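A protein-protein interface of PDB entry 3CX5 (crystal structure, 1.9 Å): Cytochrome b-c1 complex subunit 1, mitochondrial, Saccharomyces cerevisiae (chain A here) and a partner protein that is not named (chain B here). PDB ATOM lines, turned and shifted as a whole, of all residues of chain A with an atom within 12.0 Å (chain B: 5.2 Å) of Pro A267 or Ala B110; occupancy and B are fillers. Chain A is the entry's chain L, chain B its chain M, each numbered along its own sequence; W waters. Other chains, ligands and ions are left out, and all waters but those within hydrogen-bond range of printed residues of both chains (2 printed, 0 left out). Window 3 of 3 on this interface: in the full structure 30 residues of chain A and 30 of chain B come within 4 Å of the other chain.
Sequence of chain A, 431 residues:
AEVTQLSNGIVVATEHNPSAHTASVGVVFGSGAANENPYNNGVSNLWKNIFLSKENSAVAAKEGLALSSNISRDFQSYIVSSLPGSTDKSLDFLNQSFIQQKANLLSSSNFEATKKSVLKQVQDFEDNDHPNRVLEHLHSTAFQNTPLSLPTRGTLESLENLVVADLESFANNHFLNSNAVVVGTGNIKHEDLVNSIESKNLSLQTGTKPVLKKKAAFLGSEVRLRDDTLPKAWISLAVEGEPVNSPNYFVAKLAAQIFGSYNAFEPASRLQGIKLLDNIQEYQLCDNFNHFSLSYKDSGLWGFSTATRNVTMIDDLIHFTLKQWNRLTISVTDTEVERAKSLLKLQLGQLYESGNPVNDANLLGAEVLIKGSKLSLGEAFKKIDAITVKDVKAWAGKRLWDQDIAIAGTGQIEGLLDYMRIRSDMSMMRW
The guanidinium group (NH1) of Arg B37 lies within salt-bridge range of the side-chain carboxylate (OE2) of Glu A266 (2.7 Å).
The side-chain amide oxygen (OD1) of Asn A263 lies within hydrogen-bond range of the side-chain hydroxyl (OH) of Tyr B113 (3.5 Å).
OG of Ser A269 is in hydrogen-bond range of N of Asn A263, at 2.8 Å.
The backbone carbonyl oxygen (O) of Ala A264 is in hydrogen-bond range of the guanidinium group (NH2) of Arg A270, 3.4 Å away.
The guanidinium group (NH2) of Arg B37 is in salt-bridge range of the side-chain carboxylate (OD1) of Asp B114 (2.8 Å).
The side-chain amide nitrogen (ND2) of Asn A263 sits close to the backbone NH (N) of Phe A265 (3.0 Å).
Tyr B113 touches Phe A265 (CG to CB, 3.5 Å).
CE2 of Tyr B113 touches OE1 of Glu A266, 3.7 Å away.
Pro A267 touches Arg B37 (CD to NH1, 3.8 Å).
Pro A267 touches Ala B110.
Ser B106 touches Arg A270.
Of the printed residues of chain B, Pro A267 touches Arg B37 (3.8 Å) and Ala B110 (3.8 Å).
Ala B110 touches just one residue of chain A: Pro A267 (3.8 Å).
Ser B106 touches just one residue of chain A: Arg A270 (3.6 Å).
No residue of chain A comes within 4 Å of Pro B109.
No residue of chain A comes within 4 Å of Ala B111.
Of the printed residues of chain B, Asn A263 touches Tyr B113 (3.5 Å).
Of the printed residues of chain B, Phe A265 touches Tyr B113.
Printed residues of chain B within 4 Å of Arg A270: Ser B106 (3.6 Å).
The nearest printed residue of chain B that does not touch Pro A267 is Gln B41 (4.003 Å).
Of the 21 printed residues of chain A, 5 touch a printed residue of chain B.
Printed residues of chain A that touch a printed residue of chain B: Asn A263, Phe A265, Glu A266, Pro A267 and Arg A270.
Hydrophobic or aromatic side chains of chain A within 4 Å of the printed part of chain B: Phe A265 and Pro A267.
Hydrophobic or aromatic side chains of chain B within 4 Å of the printed part of chain A: Ala B110 and Tyr B113.
Among the printed residues, Asp or Glu carboxylates within 4 Å of a Lys or Arg side-chain nitrogen of the other chain: Glu A266 with Arg B37 (2.7 Å).
Water W2 bridges the guanidinium group (NH2) of Arg A270 and the backbone carbonyl oxygen (O) of Ser B106.
Water W1 bridges O of Phe A265 (2.9 Å) and N of Ala B110 (3.4 Å).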
ATOM      1  N   SER A 261      34.132  14.408  13.849  1.00  0.00           N
ATOM      2  CA  SER A 261      32.899  14.074  13.149  1.00  0.00           C
ATOM      3  C   SER A 261      32.129  13.037  13.956  1.00  0.00           C
ATOM      4  O   SER A 261      32.708  12.336  14.782  1.00  0.00           O
ATOM      5  CB  SER A 261      33.191  13.611  11.713  1.00  0.00           C
ATOM      6  OG  SER A 261      33.904  12.392  11.686  1.00  0.00           O
ATOM      7  N   TYR A 262      30.828  12.936  13.706  1.00  0.00           N
ATOM      8  CA  TYR A 262      29.975  12.055  14.479  1.00  0.00           C
ATOM      9  C   TYR A 262      28.816  11.481  13.681  1.00  0.00           C
ATOM     10  O   TYR A 262      28.289  12.135  12.788  1.00  0.00           O
ATOM     11  CB  TYR A 262      29.441  12.869  15.669  1.00  0.00           C
ATOM     12  CG  TYR A 262      28.287  12.269  16.441  1.00  0.00           C
ATOM     13  CD1 TYR A 262      27.009  12.832  16.371  1.00  0.00           C
ATOM     14  CD2 TYR A 262      28.479  11.175  17.286  1.00  0.00           C
ATOM     15  CE1 TYR A 262      25.949  12.322  17.130  1.00  0.00           C
ATOM     16  CE2 TYR A 262      27.431  10.657  18.050  1.00  0.00           C
ATOM     17  CZ  TYR A 262      26.170  11.235  17.969  1.00  0.00           C
ATOM     18  OH  TYR A 262      25.133  10.726  18.727  1.00  0.00           O
ATOM     19  N   ASN A 263      28.438  10.248  14.014  1.00  0.00           N
ATOM     20  CA  ASN A 263      27.318   9.568  13.375  1.00  0.00           C
ATOM     21  C   ASN A 263      26.546   8.882  14.501  1.00  0.00           C
ATOM     22  O   ASN A 263      26.978   7.855  15.034  1.00  0.00           O
ATOM     23  CB  ASN A 263      27.806   8.541  12.343  1.00  0.00           C
ATOM     24  CG  ASN A 263      26.658   7.902  11.551  1.00  0.00           C
ATOM     25  OD1 ASN A 263      26.872   7.356  10.469  1.00  0.00           O
ATOM     26  ND2 ASN A 263      25.447   7.960  12.089  1.00  0.00           N
ATOM     27  N   ALA A 264      25.398   9.461  14.847  1.00  0.00           N
ATOM     28  CA  ALA A 264      24.543   8.956  15.921  1.00  0.00           C
ATOM     29  C   ALA A 264      24.126   7.490  15.801  1.00  0.00           C
ATOM     30  O   ALA A 264      23.778   6.853  16.796  1.00  0.00           O
ATOM     31  CB  ALA A 264      23.307   9.840  16.051  1.00  0.00           C
ATOM     32  N   PHE A 265      24.175   6.949  14.591  1.00  0.00           N
ATOM     33  CA  PHE A 265      23.762   5.568  14.371  1.00  0.00           C
ATOM     34  C   PHE A 265      24.869   4.529  14.527  1.00  0.00           C
ATOM     35  O   PHE A 265      24.583   3.339  14.643  1.00  0.00           O
ATOM     36  CB  PHE A 265      23.071   5.443  13.012  1.00  0.00           C
ATOM     37  CG  PHE A 265      21.819   6.270  12.898  1.00  0.00           C
ATOM     38  CD1 PHE A 265      21.823   7.466  12.181  1.00  0.00           C
ATOM     39  CD2 PHE A 265      20.642   5.867  13.532  1.00  0.00           C
ATOM     40  CE1 PHE A 265      20.671   8.256  12.095  1.00  0.00           C
ATOM     41  CE2 PHE A 265      19.485   6.648  13.454  1.00  0.00           C
ATOM     42  CZ  PHE A 265      19.502   7.846  12.733  1.00  0.00           C
ATOM     43  N   GLU A 266      26.120   4.987  14.547  1.00  0.00           N
ATOM     44  CA  GLU A 266      27.282   4.111  14.703  1.00  0.00           C
ATOM     45  C   GLU A 266      27.656   4.026  16.180  1.00  0.00           C
ATOM     46  O   GLU A 266      28.085   5.014  16.773  1.00  0.00           O
ATOM     47  CB  GLU A 266      28.466   4.648  13.892  1.00  0.00           C
ATOM     48  CG  GLU A 266      28.302   4.508  12.379  1.00  0.00           C
ATOM     49  CD  GLU A 266      28.329   3.054  11.905  1.00  0.00           C
ATOM     50  OE1 GLU A 266      27.768   2.770  10.831  1.00  0.00           O
ATOM     51  OE2 GLU A 266      28.906   2.190  12.602  1.00  0.00           O
ATOM     52  N   PRO A 267      27.512   2.837  16.790  1.00  0.00           N
ATOM     53  CA  PRO A 267      27.831   2.631  18.211  1.00  0.00           C
ATOM     54  C   PRO A 267      29.182   3.199  18.678  1.00  0.00           C
ATOM     55  O   PRO A 267      29.253   3.872  19.708  1.00  0.00           O
ATOM     56  CB  PRO A 267      27.775   1.108  18.351  1.00  0.00           C
ATOM     57  CG  PRO A 267      26.711   0.727  17.367  1.00  0.00           C
ATOM     58  CD  PRO A 267      27.068   1.579  16.163  1.00  0.00           C
ATOM     59  N   ALA A 268      30.239   2.953  17.908  1.00  0.00           N
ATOM     60  CA  ALA A 268      31.573   3.433  18.271  1.00  0.00           C
ATOM     61  C   ALA A 268      31.720   4.945  18.155  1.00  0.00           C
ATOM     62  O   ALA A 268      32.528   5.551  18.865  1.00  0.00           O
ATOM     63  CB  ALA A 268      32.641   2.735  17.430  1.00  0.00           C
ATOM     64  N   SER A 269      30.968   5.546  17.235  1.00  0.00           N
ATOM     65  CA  SER A 269      31.016   6.991  17.029  1.00  0.00           C
ATOM     66  C   SER A 269      30.505   7.719  18.276  1.00  0.00           C
ATOM     67  O   SER A 269      30.999   8.795  18.624  1.00  0.00           O
ATOM     68  CB  SER A 269      30.178   7.385  15.804  1.00  0.00           C
ATOM     69  OG  SER A 269      30.382   8.748  15.456  1.00  0.00           O
ATOM     70  N   ARG A 270      29.561   7.089  18.972  1.00  0.00           N
ATOM     71  CA  ARG A 270      28.966   7.657  20.178  1.00  0.00           C
ATOM     72  C   ARG A 270      29.892   7.588  21.393  1.00  0.00           C
ATOM     73  O   ARG A 270      29.653   8.257  22.398  1.00  0.00           O
ATOM     74  CB  ARG A 270      27.653   6.936  20.511  1.00  0.00           C
ATOM     75  CG  ARG A 270      26.614   6.940  19.396  1.00  0.00           C
ATOM     76  CD  ARG A 270      25.231   6.579  19.934  1.00  0.00           C
ATOM     77  NE  ARG A 270      25.232   5.265  20.561  1.00  0.00           N
ATOM     78  CZ  ARG A 270      24.587   4.198  20.091  1.00  0.00           C
ATOM     79  NH1 ARG A 270      24.666   3.036  20.739  1.00  0.00           N
ATOM     80  NH2 ARG A 270      23.847   4.291  18.988  1.00  0.00           N
ATOM     81  N   LEU A 271      30.942   6.779  21.296  1.00  0.00           N
ATOM     82  CA  LEU A 271      31.880   6.604  22.397  1.00  0.00           C
ATOM     83  C   LEU A 271      33.148   7.453  22.319  1.00  0.00           C
ATOM     84  O   LEU A 271      34.001   7.367  23.200  1.00  0.00           O
ATOM     85  CB  LEU A 271      32.253   5.120  22.511  1.00  0.00           C
ATOM     86  CG  LEU A 271      31.088   4.141  22.734  1.00  0.00           C
ATOM     87  CD1 LEU A 271      31.568   2.708  22.555  1.00  0.00           C
ATOM     88  CD2 LEU A 271      30.480   4.337  24.120  1.00  0.00           C
ATOM     89  N   GLN A 272      33.259   8.288  21.290  1.00  0.00           N
ATOM     90  CA  GLN A 272      34.442   9.132  21.095  1.00  0.00           C
ATOM     91  C   GLN A 272      34.750  10.100  22.236  1.00  0.00           C
ATOM     92  O   GLN A 272      33.842  10.597  22.915  1.00  0.00           O
ATOM     93  CB  GLN A 272      34.317   9.927  19.792  1.00  0.00           C
ATOM     94  CG  GLN A 272      34.285   9.087  18.516  1.00  0.00           C
ATOM     95  CD  GLN A 272      34.140   9.936  17.265  1.00  0.00           C
ATOM     96  OE1 GLN A 272      35.126  10.427  16.715  1.00  0.00           O
ATOM     97  NE2 GLN A 272      32.903  10.125  16.815  1.00  0.00           N
ATOM     98  N   GLY A 273      36.042  10.392  22.411  1.00  0.00           N
ATOM     99  CA  GLY A 273      36.487  11.312  23.443  1.00  0.00           C
ATOM    100  C   GLY A 273      36.268  12.759  23.036  1.00  0.00           C
ATOM    101  O   GLY A 273      37.221  13.543  22.915  1.00  0.00           O
ATOM    102  N   ILE A 274      35.001  13.102  22.792  1.00  0.00           N
ATOM    103  CA  ILE A 274      34.603  14.452  22.397  1.00  0.00           C
ATOM    104  C   ILE A 274      33.580  14.930  23.426  1.00  0.00           C
ATOM    105  O   ILE A 274      32.508  14.340  23.557  1.00  0.00           O
ATOM    106  CB  ILE A 274      33.974  14.456  20.980  1.00  0.00           C
ATOM    107  CG1 ILE A 274      34.973  13.889  19.959  1.00  0.00           C
ATOM    108  CG2 ILE A 274      33.572  15.882  20.581  1.00  0.00           C
ATOM    109  CD1 ILE A 274      34.343  13.487  18.627  1.00  0.00           C
ATOM    110  N   LEU A 277      29.852  15.571  22.701  1.00  0.00           N
ATOM    111  CA  LEU A 277      28.972  14.406  22.661  1.00  0.00           C
ATOM    112  C   LEU A 277      28.143  14.181  23.923  1.00  0.00           C
ATOM    113  O   LEU A 277      27.074  13.591  23.860  1.00  0.00           O
ATOM    114  CB  LEU A 277      29.754  13.148  22.279  1.00  0.00           C
ATOM    115  CG  LEU A 277      30.329  13.156  20.857  1.00  0.00           C
ATOM    116  CD1 LEU A 277      30.871  11.774  20.526  1.00  0.00           C
ATOM    117  CD2 LEU A 277      29.262  13.541  19.850  1.00  0.00           C
ATOM    118  N   ASP A 278      28.626  14.656  25.067  1.00  0.00           N
ATOM    119  CA  ASP A 278      27.870  14.519  26.311  1.00  0.00           C
ATOM    120  C   ASP A 278      26.634  15.417  26.273  1.00  0.00           C
ATOM    121  O   ASP A 278      25.557  15.025  26.735  1.00  0.00           O
ATOM    122  CB  ASP A 278      28.729  14.896  27.515  1.00  0.00           C
ATOM    123  CG  ASP A 278      29.783  13.859  27.827  1.00  0.00           C
ATOM    124  OD1 ASP A 278      30.800  14.226  28.456  1.00  0.00           O
ATOM    125  OD2 ASP A 278      29.595  12.677  27.454  1.00  0.00           O
ATOM    126  N   GLN A 281      23.908  14.082  22.995  1.00  0.00           N
ATOM    127  CA  GLN A 281      23.272  12.774  22.972  1.00  0.00           C
ATOM    128  C   GLN A 281      22.053  12.596  23.876  1.00  0.00           C
ATOM    129  O   GLN A 281      21.163  11.804  23.561  1.00  0.00           O
ATOM    130  CB  GLN A 281      24.309  11.677  23.204  1.00  0.00           C
ATOM    131  CG  GLN A 281      25.350  11.642  22.081  1.00  0.00           C
ATOM    132  CD  GLN A 281      26.265  10.432  22.134  1.00  0.00           C
ATOM    133  OE1 GLN A 281      26.436   9.737  21.138  1.00  0.00           O
ATOM    134  NE2 GLN A 281      26.875  10.193  23.284  1.00  0.00           N
ATOM    135  N   GLN A 284      19.319  13.804  21.822  1.00  0.00           N
ATOM    136  CA  GLN A 284      19.671  13.484  20.438  1.00  0.00           C
ATOM    137  C   GLN A 284      19.460  14.669  19.500  1.00  0.00           C
ATOM    138  O   GLN A 284      18.555  14.693  18.665  1.00  0.00           O
ATOM    139  CB  GLN A 284      18.954  12.225  19.947  1.00  0.00           C
ATOM    140  CG  GLN A 284      19.771  11.446  18.891  1.00  0.00           C
ATOM    141  CD  GLN A 284      21.217  11.159  19.337  1.00  0.00           C
ATOM    142  OE1 GLN A 284      21.460  10.336  20.227  1.00  0.00           O
ATOM    143  NE2 GLN A 284      22.175  11.850  18.723  1.00  0.00           N
ATOM    144  N   CYS A 286      21.210  15.692  16.944  1.00  0.00           N
ATOM    145  CA  CYS A 286      21.485  15.537  15.517  1.00  0.00           C
ATOM    146  C   CYS A 286      21.755  14.092  15.114  1.00  0.00           C
ATOM    147  O   CYS A 286      21.944  13.224  15.964  1.00  0.00           O
ATOM    148  CB  CYS A 286      22.681  16.408  15.099  1.00  0.00           C
ATOM    149  SG  CYS A 286      24.290  15.820  15.697  1.00  0.00           S
ATOM    150  N   ASP A 287      21.720  13.837  13.809  1.00  0.00           N
ATOM    151  CA  ASP A 287      22.009  12.511  13.273  1.00  0.00           C
ATOM    152  C   ASP A 287      23.511  12.406  12.986  1.00  0.00           C
ATOM    153  O   ASP A 287      24.097  11.323  13.083  1.00  0.00           O
ATOM    154  CB  ASP A 287      21.224  12.255  11.988  1.00  0.00           C
ATOM    155  CG  ASP A 287      19.754  11.955  12.243  1.00  0.00           C
ATOM    156  OD1 ASP A 287      18.972  11.995  11.272  1.00  0.00           O
ATOM    157  OD2 ASP A 287      19.384  11.658  13.403  1.00  0.00           O
ATOM    158  N   ASN A 288      24.122  13.538  12.640  1.00  0.00           N
ATOM    159  CA  ASN A 288      25.550  13.582  12.347  1.00  0.00           C
ATOM    160  C   ASN A 288      26.099  14.994  12.273  1.00  0.00           C
ATOM    161  O   ASN A 288      25.346  15.957  12.180  1.00  0.00           O
ATOM    162  CB  ASN A 288      25.865  12.870  11.017  1.00  0.00           C
ATOM    163  CG  ASN A 288      25.012  13.363   9.857  1.00  0.00           C
ATOM    164  OD1 ASN A 288      24.006  12.744   9.514  1.00  0.00           O
ATOM    165  ND2 ASN A 288      25.424  14.461   9.227  1.00  0.00           N
ATOM    166  N   ARG B  37      27.704  -6.697  13.874  1.00  0.00           N
ATOM    167  CA  ARG B  37      27.355  -5.527  14.661  1.00  0.00           C
ATOM    168  C   ARG B  37      27.814  -5.681  16.122  1.00  0.00           C
ATOM    169  O   ARG B  37      28.052  -4.684  16.803  1.00  0.00           O
ATOM    170  CB  ARG B  37      25.846  -5.313  14.578  1.00  0.00           C
ATOM    171  CG  ARG B  37      25.393  -3.920  14.180  1.00  0.00           C
ATOM    172  CD  ARG B  37      26.002  -3.414  12.884  1.00  0.00           C
ATOM    173  NE  ARG B  37      26.970  -2.356  13.159  1.00  0.00           N
ATOM    174  CZ  ARG B  37      27.005  -1.164  12.563  1.00  0.00           C
ATOM    175  NH1 ARG B  37      27.937  -0.291  12.913  1.00  0.00           N
ATOM    176  NH2 ARG B  37      26.141  -0.843  11.613  1.00  0.00           N
ATOM    177  N   GLN B  41      32.111  -4.558  20.634  1.00  0.00           N
ATOM    178  CA  GLN B  41      31.320  -4.210  21.801  1.00  0.00           C
ATOM    179  C   GLN B  41      32.256  -4.634  22.951  1.00  0.00           C
ATOM    180  O   GLN B  41      33.430  -4.934  22.714  1.00  0.00           O
ATOM    181  CB  GLN B  41      30.017  -5.018  21.838  1.00  0.00           C
ATOM    182  CG  GLN B  41      28.901  -4.481  20.941  1.00  0.00           C
ATOM    183  CD  GLN B  41      28.412  -3.102  21.358  1.00  0.00           C
ATOM    184  OE1 GLN B  41      28.183  -2.233  20.518  1.00  0.00           O
ATOM    185  NE2 GLN B  41      28.242  -2.901  22.661  1.00  0.00           N
ATOM    186  N   SER B 106      22.579  -1.377  21.713  1.00  0.00           N
ATOM    187  CA  SER B 106      23.474  -1.006  20.618  1.00  0.00           C
ATOM    188  C   SER B 106      23.389  -1.831  19.339  1.00  0.00           C
ATOM    189  O   SER B 106      23.267  -1.275  18.250  1.00  0.00           O
ATOM    190  CB  SER B 106      24.920  -1.019  21.104  1.00  0.00           C
ATOM    191  OG  SER B 106      25.069  -0.231  22.264  1.00  0.00           O
ATOM    192  N   VAL B 107      23.472  -3.153  19.481  1.00  0.00           N
ATOM    193  CA  VAL B 107      23.455  -4.055  18.340  1.00  0.00           C
ATOM    194  C   VAL B 107      22.192  -4.008  17.496  1.00  0.00           C
ATOM    195  O   VAL B 107      22.264  -3.701  16.307  1.00  0.00           O
ATOM    196  CB  VAL B 107      23.780  -5.499  18.768  1.00  0.00           C
ATOM    197  CG1 VAL B 107      23.773  -6.430  17.553  1.00  0.00           C
ATOM    198  CG2 VAL B 107      25.149  -5.530  19.442  1.00  0.00           C
ATOM    199  N   LEU B 108      21.042  -4.317  18.089  1.00  0.00           N
ATOM    200  CA  LEU B 108      19.788  -4.276  17.342  1.00  0.00           C
ATOM    201  C   LEU B 108      19.513  -2.916  16.681  1.00  0.00           C
ATOM    202  O   LEU B 108      19.203  -2.868  15.491  1.00  0.00           O
ATOM    203  CB  LEU B 108      18.604  -4.702  18.215  1.00  0.00           C
ATOM    204  CG  LEU B 108      18.476  -6.205  18.478  1.00  0.00           C
ATOM    205  CD1 LEU B 108      17.249  -6.478  19.342  1.00  0.00           C
ATOM    206  CD2 LEU B 108      18.378  -6.959  17.147  1.00  0.00           C
ATOM    207  N   PRO B 109      19.637  -1.799  17.431  1.00  0.00           N
ATOM    208  CA  PRO B 109      19.383  -0.479  16.832  1.00  0.00           C
ATOM    209  C   PRO B 109      20.285  -0.219  15.626  1.00  0.00           C
ATOM    210  O   PRO B 109      19.820   0.272  14.604  1.00  0.00           O
ATOM    211  CB  PRO B 109      19.698   0.492  17.977  1.00  0.00           C
ATOM    212  CG  PRO B 109      19.356  -0.307  19.192  1.00  0.00           C
ATOM    213  CD  PRO B 109      19.941  -1.660  18.868  1.00  0.00           C
ATOM    214  N   ALA B 110      21.566  -0.563  15.750  1.00  0.00           N
ATOM    215  CA  ALA B 110      22.523  -0.375  14.663  1.00  0.00           C
ATOM    216  C   ALA B 110      22.180  -1.236  13.442  1.00  0.00           C
ATOM    217  O   ALA B 110      22.348  -0.801  12.300  1.00  0.00           O
ATOM    218  CB  ALA B 110      23.924  -0.677  15.140  1.00  0.00           C
ATOM    219  N   ALA B 111      21.718  -2.461  13.689  1.00  0.00           N
ATOM    220  CA  ALA B 111      21.342  -3.366  12.607  1.00  0.00           C
ATOM    221  C   ALA B 111      20.064  -2.862  11.934  1.00  0.00           C
ATOM    222  O   ALA B 111      19.868  -3.075  10.734  1.00  0.00           O
ATOM    223  CB  ALA B 111      21.152  -4.786  13.133  1.00  0.00           C
ATOM    224  N   ARG B 112      19.198  -2.207  12.714  1.00  0.00           N
ATOM    225  CA  ARG B 112      17.954  -1.636  12.187  1.00  0.00           C
ATOM    226  C   ARG B 112      18.307  -0.483  11.248  1.00  0.00           C
ATOM    227  O   ARG B 112      17.679  -0.298  10.204  1.00  0.00           O
ATOM    228  CB  ARG B 112      17.064  -1.109  13.315  1.00  0.00           C
ATOM    229  CG  ARG B 112      16.231  -2.160  14.019  1.00  0.00           C
ATOM    230  CD  ARG B 112      15.332  -1.516  15.068  1.00  0.00           C
ATOM    231  NE  ARG B 112      14.382  -2.466  15.649  1.00  0.00           N
ATOM    232  CZ  ARG B 112      14.641  -3.270  16.680  1.00  0.00           C
ATOM    233  NH1 ARG B 112      13.703  -4.096  17.130  1.00  0.00           N
ATOM    234  NH2 ARG B 112      15.831  -3.250  17.268  1.00  0.00           N
ATOM    235  N   TYR B 113      19.315   0.289  11.643  1.00  0.00           N
ATOM    236  CA  TYR B 113      19.812   1.413  10.854  1.00  0.00           C
ATOM    237  C   TYR B 113      20.290   0.875   9.496  1.00  0.00           C
ATOM    238  O   TYR B 113      19.826   1.335   8.450  1.00  0.00           O
ATOM    239  CB  TYR B 113      20.949   2.105  11.623  1.00  0.00           C
ATOM    240  CG  TYR B 113      21.916   2.937  10.798  1.00  0.00           C
ATOM    241  CD1 TYR B 113      21.481   4.053  10.074  1.00  0.00           C
ATOM    242  CD2 TYR B 113      23.284   2.640  10.794  1.00  0.00           C
ATOM    243  CE1 TYR B 113      22.389   4.855   9.369  1.00  0.00           C
ATOM    244  CE2 TYR B 113      24.198   3.434  10.096  1.00  0.00           C
ATOM    245  CZ  TYR B 113      23.746   4.540   9.388  1.00  0.00           C
ATOM    246  OH  TYR B 113      24.654   5.334   8.713  1.00  0.00           O
ATOM    247  N   ASP B 114      21.167  -0.132   9.524  1.00  0.00           N
ATOM    248  CA  ASP B 114      21.689  -0.749   8.297  1.00  0.00           C
ATOM    249  C   ASP B 114      20.559  -1.243   7.395  1.00  0.00           C
ATOM    250  O   ASP B 114      20.568  -1.002   6.186  1.00  0.00           O
ATOM    251  CB  ASP B 114      22.597  -1.933   8.619  1.00  0.00           C
ATOM    252  CG  ASP B 114      23.837  -1.538   9.396  1.00  0.00           C
ATOM    253  OD1 ASP B 114      24.411  -2.420  10.060  1.00  0.00           O
ATOM    254  OD2 ASP B 114      24.241  -0.357   9.358  1.00  0.00           O
HETATM  255  O   HOH W   1      22.028   2.764  15.944  1.00  0.00           O
HETATM  256  O   HOH W   2      23.200   1.605  18.542  1.00  0.00           O
